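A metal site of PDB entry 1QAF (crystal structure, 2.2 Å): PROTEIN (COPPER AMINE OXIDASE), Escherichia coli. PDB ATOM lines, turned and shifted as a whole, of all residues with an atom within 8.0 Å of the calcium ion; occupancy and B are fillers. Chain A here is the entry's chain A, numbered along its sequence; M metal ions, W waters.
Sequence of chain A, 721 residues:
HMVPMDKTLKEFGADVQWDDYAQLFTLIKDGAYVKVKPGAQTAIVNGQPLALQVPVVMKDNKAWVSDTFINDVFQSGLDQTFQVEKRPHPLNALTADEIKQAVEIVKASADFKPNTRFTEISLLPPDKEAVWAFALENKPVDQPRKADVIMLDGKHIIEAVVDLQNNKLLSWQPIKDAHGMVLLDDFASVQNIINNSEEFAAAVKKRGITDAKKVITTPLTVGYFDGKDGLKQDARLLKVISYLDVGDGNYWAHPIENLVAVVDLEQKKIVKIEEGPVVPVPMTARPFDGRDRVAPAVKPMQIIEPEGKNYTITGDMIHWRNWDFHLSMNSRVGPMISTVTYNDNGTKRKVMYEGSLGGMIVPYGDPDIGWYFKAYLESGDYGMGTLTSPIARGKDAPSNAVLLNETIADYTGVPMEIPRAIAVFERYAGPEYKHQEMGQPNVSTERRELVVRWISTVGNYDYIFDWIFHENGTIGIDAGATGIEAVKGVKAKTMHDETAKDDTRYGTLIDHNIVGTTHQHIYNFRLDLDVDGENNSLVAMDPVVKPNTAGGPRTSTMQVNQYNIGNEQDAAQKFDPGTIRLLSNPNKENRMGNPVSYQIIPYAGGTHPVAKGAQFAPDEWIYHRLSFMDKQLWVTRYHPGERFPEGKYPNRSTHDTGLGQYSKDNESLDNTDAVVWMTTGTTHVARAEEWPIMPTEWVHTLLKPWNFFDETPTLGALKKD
O of Glu 354 sits at hydrogen-bond distance from N of Asp 528 (2.8 Å).
N of Tyr 638 sits at hydrogen-bond distance from O of Asp 673, at 3.0 Å.
The backbone NH (N) of Tyr 353 sits at hydrogen-bond distance from the backbone carbonyl oxygen (O) of Asp 528 (2.9 Å).
NZ of Lys 128 is in salt-bridge range of OD2 of Asp 528, at 2.7 Å.
The side-chain amino group of Lys 128 lies within salt-bridge range of the side-chain carboxylate of Asp 530 (3.0 Å).
O of Val 351 is in hydrogen-bond range of N of Asp 530, 2.8 Å away.
The side-chain carboxylate (OD2) of Asp 530 is in hydrogen-bond range of the indole nitrogen (NE1) of Trp 132, at 2.8 Å.
NZ of Lys 128 lies within salt-bridge range of OD2 of Asp 673 (2.8 Å).
Lys 128 touches the calcium ion.
Six residues have an atom within 4 Å of the calcium ion: Lys 128, Asp 528, Leu 529, Asp 530, Asp 673 and Ala 674.
The nearest printed residue that does not touch the calcium ion is Glu 534 (4.6 Å).
The calcium ion is bound by OD1 of Asp 530 (2.3 Å), OD1 of Asp 673 (2.4 Å), O of Ala 674 (2.4 Å), OD1 of Asp 528 (2.4 Å), O of Leu 529 (2.5 Å) and water W1 (2.6 Å).
Water W1 lies within hydrogen-bond range of the backbone carbonyl oxygen of Glu 534 (2.7 Å), the side-chain amide nitrogen of Asn 536 (2.8 Å) and the backbone NH of Ala 674 (3.0 Å).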
ATOM      1  N   LYS A 128      -4.175  20.640 -10.930  1.00  0.00           N
ATOM      2  CA  LYS A 128      -3.891  21.607  -9.900  1.00  0.00           C
ATOM      3  C   LYS A 128      -3.055  21.041  -8.756  1.00  0.00           C
ATOM      4  O   LYS A 128      -2.049  21.601  -8.292  1.00  0.00           O
ATOM      5  CB  LYS A 128      -5.261  22.128  -9.405  1.00  0.00           C
ATOM      6  CG  LYS A 128      -5.201  23.089  -8.224  1.00  0.00           C
ATOM      7  CD  LYS A 128      -6.403  24.025  -8.035  1.00  0.00           C
ATOM      8  CE  LYS A 128      -6.313  24.835  -6.735  1.00  0.00           C
ATOM      9  NZ  LYS A 128      -7.375  25.874  -6.672  1.00  0.00           N
ATOM     10  N   TRP A 132       0.589  22.133  -7.630  1.00  0.00           N
ATOM     11  CA  TRP A 132       1.034  22.692  -6.339  1.00  0.00           C
ATOM     12  C   TRP A 132       2.103  21.795  -5.738  1.00  0.00           C
ATOM     13  O   TRP A 132       3.000  22.341  -5.090  1.00  0.00           O
ATOM     14  CB  TRP A 132      -0.158  22.778  -5.383  1.00  0.00           C
ATOM     15  CG  TRP A 132      -0.950  24.064  -5.281  1.00  0.00           C
ATOM     16  CD1 TRP A 132      -2.287  24.277  -5.342  1.00  0.00           C
ATOM     17  CD2 TRP A 132      -0.362  25.350  -5.036  1.00  0.00           C
ATOM     18  NE1 TRP A 132      -2.616  25.603  -5.173  1.00  0.00           N
ATOM     19  CE2 TRP A 132      -1.411  26.268  -4.947  1.00  0.00           C
ATOM     20  CE3 TRP A 132       0.962  25.759  -4.831  1.00  0.00           C
ATOM     21  CZ2 TRP A 132      -1.168  27.627  -4.742  1.00  0.00           C
ATOM     22  CZ3 TRP A 132       1.241  27.098  -4.612  1.00  0.00           C
ATOM     23  CH2 TRP A 132       0.150  27.981  -4.582  1.00  0.00           C
ATOM     24  N   VAL A 351      -1.339  31.331  -1.605  1.00  0.00           N
ATOM     25  CA  VAL A 351      -2.176  32.522  -1.663  1.00  0.00           C
ATOM     26  C   VAL A 351      -3.078  32.372  -2.901  1.00  0.00           C
ATOM     27  O   VAL A 351      -4.303  32.422  -2.805  1.00  0.00           O
ATOM     28  CB  VAL A 351      -1.421  33.858  -1.691  1.00  0.00           C
ATOM     29  CG1 VAL A 351      -2.357  35.036  -1.859  1.00  0.00           C
ATOM     30  CG2 VAL A 351      -0.620  34.017  -0.417  1.00  0.00           C
ATOM     31  N   MET A 352      -2.465  32.192  -4.066  1.00  0.00           N
ATOM     32  CA  MET A 352      -3.265  32.043  -5.271  1.00  0.00           C
ATOM     33  C   MET A 352      -2.725  30.992  -6.237  1.00  0.00           C
ATOM     34  O   MET A 352      -1.558  31.077  -6.668  1.00  0.00           O
ATOM     35  CB  MET A 352      -3.366  33.428  -5.933  1.00  0.00           C
ATOM     36  CG  MET A 352      -4.242  33.451  -7.170  1.00  0.00           C
ATOM     37  SD  MET A 352      -4.577  35.091  -7.838  1.00  0.00           S
ATOM     38  CE  MET A 352      -2.941  35.554  -8.439  1.00  0.00           C
ATOM     39  N   TYR A 353      -3.547  30.028  -6.658  1.00  0.00           N
ATOM     40  CA  TYR A 353      -3.181  28.996  -7.609  1.00  0.00           C
ATOM     41  C   TYR A 353      -3.064  29.636  -9.000  1.00  0.00           C
ATOM     42  O   TYR A 353      -2.097  29.410  -9.684  1.00  0.00           O
ATOM     43  CB  TYR A 353      -4.160  27.823  -7.718  1.00  0.00           C
ATOM     44  CG  TYR A 353      -3.657  26.838  -8.790  1.00  0.00           C
ATOM     45  CD1 TYR A 353      -2.471  26.121  -8.597  1.00  0.00           C
ATOM     46  CD2 TYR A 353      -4.399  26.625  -9.939  1.00  0.00           C
ATOM     47  CE1 TYR A 353      -2.071  25.222  -9.589  1.00  0.00           C
ATOM     48  CE2 TYR A 353      -4.003  25.753 -10.943  1.00  0.00           C
ATOM     49  CZ  TYR A 353      -2.814  25.066 -10.759  1.00  0.00           C
ATOM     50  OH  TYR A 353      -2.357  24.193 -11.716  1.00  0.00           O
ATOM     51  N   GLU A 354      -4.008  30.408  -9.485  1.00  0.00           N
ATOM     52  CA  GLU A 354      -3.899  31.032 -10.789  1.00  0.00           C
ATOM     53  C   GLU A 354      -4.810  32.267 -10.796  1.00  0.00           C
ATOM     54  O   GLU A 354      -5.946  32.231 -10.318  1.00  0.00           O
ATOM     55  CB  GLU A 354      -4.510  30.246 -11.972  1.00  0.00           C
ATOM     56  CG  GLU A 354      -3.930  28.888 -12.241  1.00  0.00           C
ATOM     57  CD  GLU A 354      -4.673  28.195 -13.387  1.00  0.00           C
ATOM     58  OE1 GLU A 354      -4.251  28.492 -14.507  1.00  0.00           O
ATOM     59  OE2 GLU A 354      -5.638  27.406 -13.253  1.00  0.00           O
ATOM     60  N   ARG A 526     -10.373  36.643 -13.004  1.00  0.00           N
ATOM     61  CA  ARG A 526     -10.640  35.308 -12.473  1.00  0.00           C
ATOM     62  C   ARG A 526      -9.432  35.035 -11.572  1.00  0.00           C
ATOM     63  O   ARG A 526      -8.301  34.934 -12.076  1.00  0.00           O
ATOM     64  CB  ARG A 526     -10.561  34.261 -13.605  1.00  0.00           C
ATOM     65  CG  ARG A 526     -10.669  32.843 -13.074  1.00  0.00           C
ATOM     66  CD  ARG A 526     -10.560  31.788 -14.187  1.00  0.00           C
ATOM     67  NE  ARG A 526     -10.707  30.442 -13.655  1.00  0.00           N
ATOM     68  CZ  ARG A 526      -9.743  29.835 -12.990  1.00  0.00           C
ATOM     69  NH1 ARG A 526      -8.572  30.445 -12.823  1.00  0.00           N
ATOM     70  NH2 ARG A 526      -9.976  28.643 -12.502  1.00  0.00           N
ATOM     71  N   LEU A 527      -9.689  34.910 -10.289  1.00  0.00           N
ATOM     72  CA  LEU A 527      -8.721  34.664  -9.257  1.00  0.00           C
ATOM     73  C   LEU A 527      -8.953  33.453  -8.377  1.00  0.00           C
ATOM     74  O   LEU A 527      -9.645  33.396  -7.328  1.00  0.00           O
ATOM     75  CB  LEU A 527      -8.659  35.910  -8.308  1.00  0.00           C
ATOM     76  CG  LEU A 527      -8.748  37.252  -9.068  1.00  0.00           C
ATOM     77  CD1 LEU A 527      -9.015  38.384  -8.060  1.00  0.00           C
ATOM     78  CD2 LEU A 527      -7.368  37.410  -9.740  1.00  0.00           C
ATOM     79  N   ASP A 528      -8.286  32.397  -8.825  1.00  0.00           N
ATOM     80  CA  ASP A 528      -8.374  31.131  -8.072  1.00  0.00           C
ATOM     81  C   ASP A 528      -7.497  31.262  -6.841  1.00  0.00           C
ATOM     82  O   ASP A 528      -6.370  30.752  -6.804  1.00  0.00           O
ATOM     83  CB  ASP A 528      -7.947  29.944  -8.946  1.00  0.00           C
ATOM     84  CG  ASP A 528      -7.874  28.635  -8.207  1.00  0.00           C
ATOM     85  OD1 ASP A 528      -8.348  28.523  -7.051  1.00  0.00           O
ATOM     86  OD2 ASP A 528      -7.327  27.614  -8.676  1.00  0.00           O
ATOM     87  N   LEU A 529      -7.977  31.948  -5.794  1.00  0.00           N
ATOM     88  CA  LEU A 529      -7.252  32.126  -4.546  1.00  0.00           C
ATOM     89  C   LEU A 529      -7.270  30.839  -3.722  1.00  0.00           C
ATOM     90  O   LEU A 529      -8.347  30.270  -3.766  1.00  0.00           O
ATOM     91  CB  LEU A 529      -7.921  33.200  -3.624  1.00  0.00           C
ATOM     92  CG  LEU A 529      -7.856  34.639  -4.211  1.00  0.00           C
ATOM     93  CD1 LEU A 529      -8.507  35.749  -3.388  1.00  0.00           C
ATOM     94  CD2 LEU A 529      -6.377  35.013  -4.363  1.00  0.00           C
ATOM     95  N   ASP A 530      -6.220  30.395  -3.054  1.00  0.00           N
ATOM     96  CA  ASP A 530      -6.208  29.172  -2.248  1.00  0.00           C
ATOM     97  C   ASP A 530      -5.595  29.781  -0.965  1.00  0.00           C
ATOM     98  O   ASP A 530      -4.379  29.861  -0.752  1.00  0.00           O
ATOM     99  CB  ASP A 530      -5.389  28.064  -2.845  1.00  0.00           C
ATOM    100  CG  ASP A 530      -5.940  27.278  -4.005  1.00  0.00           C
ATOM    101  OD1 ASP A 530      -7.115  27.381  -4.345  1.00  0.00           O
ATOM    102  OD2 ASP A 530      -5.213  26.466  -4.651  1.00  0.00           O
ATOM    103  N   VAL A 531      -6.491  30.274  -0.096  1.00  0.00           N
ATOM    104  CA  VAL A 531      -6.042  30.925   1.128  1.00  0.00           C
ATOM    105  C   VAL A 531      -5.401  29.978   2.130  1.00  0.00           C
ATOM    106  O   VAL A 531      -6.222  29.455   2.876  1.00  0.00           O
ATOM    107  CB  VAL A 531      -7.120  31.760   1.820  1.00  0.00           C
ATOM    108  CG1 VAL A 531      -6.659  32.416   3.121  1.00  0.00           C
ATOM    109  CG2 VAL A 531      -7.565  32.806   0.784  1.00  0.00           C
ATOM    110  N   GLY A 533      -4.467  27.213   1.651  1.00  0.00           N
ATOM    111  CA  GLY A 533      -4.899  25.839   1.417  1.00  0.00           C
ATOM    112  C   GLY A 533      -6.056  25.950   0.435  1.00  0.00           C
ATOM    113  O   GLY A 533      -6.585  27.050   0.223  1.00  0.00           O
ATOM    114  N   GLU A 534      -6.408  24.803  -0.111  1.00  0.00           N
ATOM    115  CA  GLU A 534      -7.505  24.669  -1.068  1.00  0.00           C
ATOM    116  C   GLU A 534      -8.893  24.910  -0.495  1.00  0.00           C
ATOM    117  O   GLU A 534      -9.751  25.582  -1.088  1.00  0.00           O
ATOM    118  CB  GLU A 534      -7.421  23.182  -1.463  1.00  0.00           C
ATOM    119  CG  GLU A 534      -8.731  22.462  -1.476  1.00  0.00           C
ATOM    120  CD  GLU A 534      -9.040  21.634  -2.678  1.00  0.00           C
ATOM    121  OE1 GLU A 534      -8.089  21.503  -3.464  1.00  0.00           O
ATOM    122  OE2 GLU A 534      -9.930  20.942  -3.185  1.00  0.00           O
ATOM    123  N   ASN A 535      -9.180  24.367   0.668  1.00  0.00           N
ATOM    124  CA  ASN A 535     -10.506  24.493   1.282  1.00  0.00           C
ATOM    125  C   ASN A 535     -10.788  25.779   1.997  1.00  0.00           C
ATOM    126  O   ASN A 535     -10.236  26.024   3.051  1.00  0.00           O
ATOM    127  CB  ASN A 535     -10.718  23.227   2.108  1.00  0.00           C
ATOM    128  CG  ASN A 535     -10.665  21.954   1.295  1.00  0.00           C
ATOM    129  OD1 ASN A 535     -11.099  21.859   0.157  1.00  0.00           O
ATOM    130  ND2 ASN A 535     -10.093  20.856   1.783  1.00  0.00           N
ATOM    131  N   ASN A 536     -11.651  26.592   1.423  1.00  0.00           N
ATOM    132  CA  ASN A 536     -11.988  27.880   2.022  1.00  0.00           C
ATOM    133  C   ASN A 536     -13.509  28.071   2.009  1.00  0.00           C
ATOM    134  O   ASN A 536     -14.310  27.278   1.491  1.00  0.00           O
ATOM    135  CB  ASN A 536     -11.342  28.935   1.071  1.00  0.00           C
ATOM    136  CG  ASN A 536      -9.838  28.935   0.899  1.00  0.00           C
ATOM    137  OD1 ASN A 536      -9.025  28.371   1.692  1.00  0.00           O
ATOM    138  ND2 ASN A 536      -9.459  29.599  -0.208  1.00  0.00           N
ATOM    139  N   LEU A 583     -12.294  35.685   2.050  1.00  0.00           N
ATOM    140  CA  LEU A 583     -12.164  34.322   1.542  1.00  0.00           C
ATOM    141  C   LEU A 583     -11.317  33.808   2.697  1.00  0.00           C
ATOM    142  O   LEU A 583     -10.127  34.075   2.937  1.00  0.00           O
ATOM    143  CB  LEU A 583     -11.681  34.231   0.090  1.00  0.00           C
ATOM    144  CG  LEU A 583     -11.619  32.717  -0.259  1.00  0.00           C
ATOM    145  CD1 LEU A 583     -12.991  32.063  -0.319  1.00  0.00           C
ATOM    146  CD2 LEU A 583     -10.869  32.479  -1.555  1.00  0.00           C
ATOM    147  N   VAL A 635     -18.179  34.028  -6.769  1.00  0.00           N
ATOM    148  CA  VAL A 635     -17.359  32.972  -6.169  1.00  0.00           C
ATOM    149  C   VAL A 635     -17.966  31.646  -6.687  1.00  0.00           C
ATOM    150  O   VAL A 635     -19.171  31.412  -6.490  1.00  0.00           O
ATOM    151  CB  VAL A 635     -17.200  32.961  -4.643  1.00  0.00           C
ATOM    152  CG1 VAL A 635     -16.191  31.940  -4.140  1.00  0.00           C
ATOM    153  CG2 VAL A 635     -16.937  34.413  -4.245  1.00  0.00           C
ATOM    154  N   THR A 636     -17.153  30.824  -7.389  1.00  0.00           N
ATOM    155  CA  THR A 636     -17.725  29.559  -7.908  1.00  0.00           C
ATOM    156  C   THR A 636     -16.826  28.429  -7.453  1.00  0.00           C
ATOM    157  O   THR A 636     -15.707  28.783  -7.044  1.00  0.00           O
ATOM    158  CB  THR A 636     -17.734  29.533  -9.456  1.00  0.00           C
ATOM    159  OG1 THR A 636     -16.404  29.806  -9.982  1.00  0.00           O
ATOM    160  CG2 THR A 636     -18.740  30.603  -9.902  1.00  0.00           C
ATOM    161  N   ARG A 637     -17.303  27.191  -7.544  1.00  0.00           N
ATOM    162  CA  ARG A 637     -16.431  26.065  -7.165  1.00  0.00           C
ATOM    163  C   ARG A 637     -15.392  25.896  -8.286  1.00  0.00           C
ATOM    164  O   ARG A 637     -15.674  26.095  -9.479  1.00  0.00           O
ATOM    165  CB  ARG A 637     -17.165  24.737  -7.032  1.00  0.00           C
ATOM    166  CG  ARG A 637     -18.392  24.776  -6.140  1.00  0.00           C
ATOM    167  CD  ARG A 637     -18.902  23.343  -6.059  1.00  0.00           C
ATOM    168  NE  ARG A 637     -18.981  22.967  -4.669  1.00  0.00           N
ATOM    169  CZ  ARG A 637     -18.422  21.955  -4.039  1.00  0.00           C
ATOM    170  NH1 ARG A 637     -17.699  21.002  -4.577  1.00  0.00           N
ATOM    171  NH2 ARG A 637     -18.697  21.963  -2.729  1.00  0.00           N
ATOM    172  N   TYR A 638     -14.133  25.590  -7.959  1.00  0.00           N
ATOM    173  CA  TYR A 638     -13.058  25.415  -8.913  1.00  0.00           C
ATOM    174  C   TYR A 638     -13.397  24.279  -9.877  1.00  0.00           C
ATOM    175  O   TYR A 638     -13.842  23.273  -9.335  1.00  0.00           O
ATOM    176  CB  TYR A 638     -11.762  24.980  -8.181  1.00  0.00           C
ATOM    177  CG  TYR A 638     -10.688  24.608  -9.198  1.00  0.00           C
ATOM    178  CD1 TYR A 638      -9.997  25.513 -10.009  1.00  0.00           C
ATOM    179  CD2 TYR A 638     -10.360  23.268  -9.351  1.00  0.00           C
ATOM    180  CE1 TYR A 638      -9.058  25.123 -10.939  1.00  0.00           C
ATOM    181  CE2 TYR A 638      -9.411  22.825 -10.256  1.00  0.00           C
ATOM    182  CZ  TYR A 638      -8.781  23.773 -11.045  1.00  0.00           C
ATOM    183  OH  TYR A 638      -7.839  23.374 -11.946  1.00  0.00           O
ATOM    184  N   THR A 672     -14.687  24.546   0.597  1.00  0.00           N
ATOM    185  CA  THR A 672     -14.255  23.841  -0.615  1.00  0.00           C
ATOM    186  C   THR A 672     -13.368  24.730  -1.467  1.00  0.00           C
ATOM    187  O   THR A 672     -13.115  25.915  -1.183  1.00  0.00           O
ATOM    188  CB  THR A 672     -15.639  23.557  -1.224  1.00  0.00           C
ATOM    189  OG1 THR A 672     -15.345  22.722  -2.347  1.00  0.00           O
ATOM    190  CG2 THR A 672     -16.382  24.814  -1.564  1.00  0.00           C
ATOM    191  N   ASP A 673     -12.839  24.282  -2.572  1.00  0.00           N
ATOM    192  CA  ASP A 673     -11.984  24.982  -3.530  1.00  0.00           C
ATOM    193  C   ASP A 673     -12.804  26.075  -4.217  1.00  0.00           C
ATOM    194  O   ASP A 673     -13.694  25.901  -5.054  1.00  0.00           O
ATOM    195  CB  ASP A 673     -11.318  23.988  -4.519  1.00  0.00           C
ATOM    196  CG  ASP A 673     -10.154  24.701  -5.211  1.00  0.00           C
ATOM    197  OD1 ASP A 673      -9.943  25.942  -5.176  1.00  0.00           O
ATOM    198  OD2 ASP A 673      -9.354  24.042  -5.895  1.00  0.00           O
ATOM    199  N   ALA A 674     -12.564  27.337  -3.836  1.00  0.00           N
ATOM    200  CA  ALA A 674     -13.335  28.430  -4.422  1.00  0.00           C
ATOM    201  C   ALA A 674     -12.561  29.247  -5.456  1.00  0.00           C
ATOM    202  O   ALA A 674     -11.331  29.275  -5.337  1.00  0.00           O
ATOM    203  CB  ALA A 674     -13.585  29.421  -3.270  1.00  0.00           C
ATOM    204  N   VAL A 675     -13.260  29.889  -6.370  1.00  0.00           N
ATOM    205  CA  VAL A 675     -12.576  30.709  -7.360  1.00  0.00           C
ATOM    206  C   VAL A 675     -13.351  32.049  -7.267  1.00  0.00           C
ATOM    207  O   VAL A 675     -14.579  32.003  -7.403  1.00  0.00           O
ATOM    208  CB  VAL A 675     -12.615  30.254  -8.831  1.00  0.00           C
ATOM    209  CG1 VAL A 675     -11.882  31.237  -9.731  1.00  0.00           C
ATOM    210  CG2 VAL A 675     -12.008  28.845  -8.982  1.00  0.00           C
ATOM    211  N   VAL A 676     -12.664  33.172  -7.052  1.00  0.00           N
ATOM    212  CA  VAL A 676     -13.282  34.496  -6.961  1.00  0.00           C
ATOM    213  C   VAL A 676     -13.137  35.229  -8.285  1.00  0.00           C
ATOM    214  O   VAL A 676     -12.077  35.139  -8.929  1.00  0.00           O
ATOM    215  CB  VAL A 676     -12.397  35.306  -5.981  1.00  0.00           C
ATOM    216  CG1 VAL A 676     -12.895  36.763  -5.966  1.00  0.00           C
ATOM    217  CG2 VAL A 676     -12.423  34.663  -4.586  1.00  0.00           C
HETATM  218 CA    CA M   1      -9.232  28.195  -4.822  1.00  0.00          CA
HETATM  219  O   HOH W   1     -10.015  27.901  -2.345  1.00  0.00           O
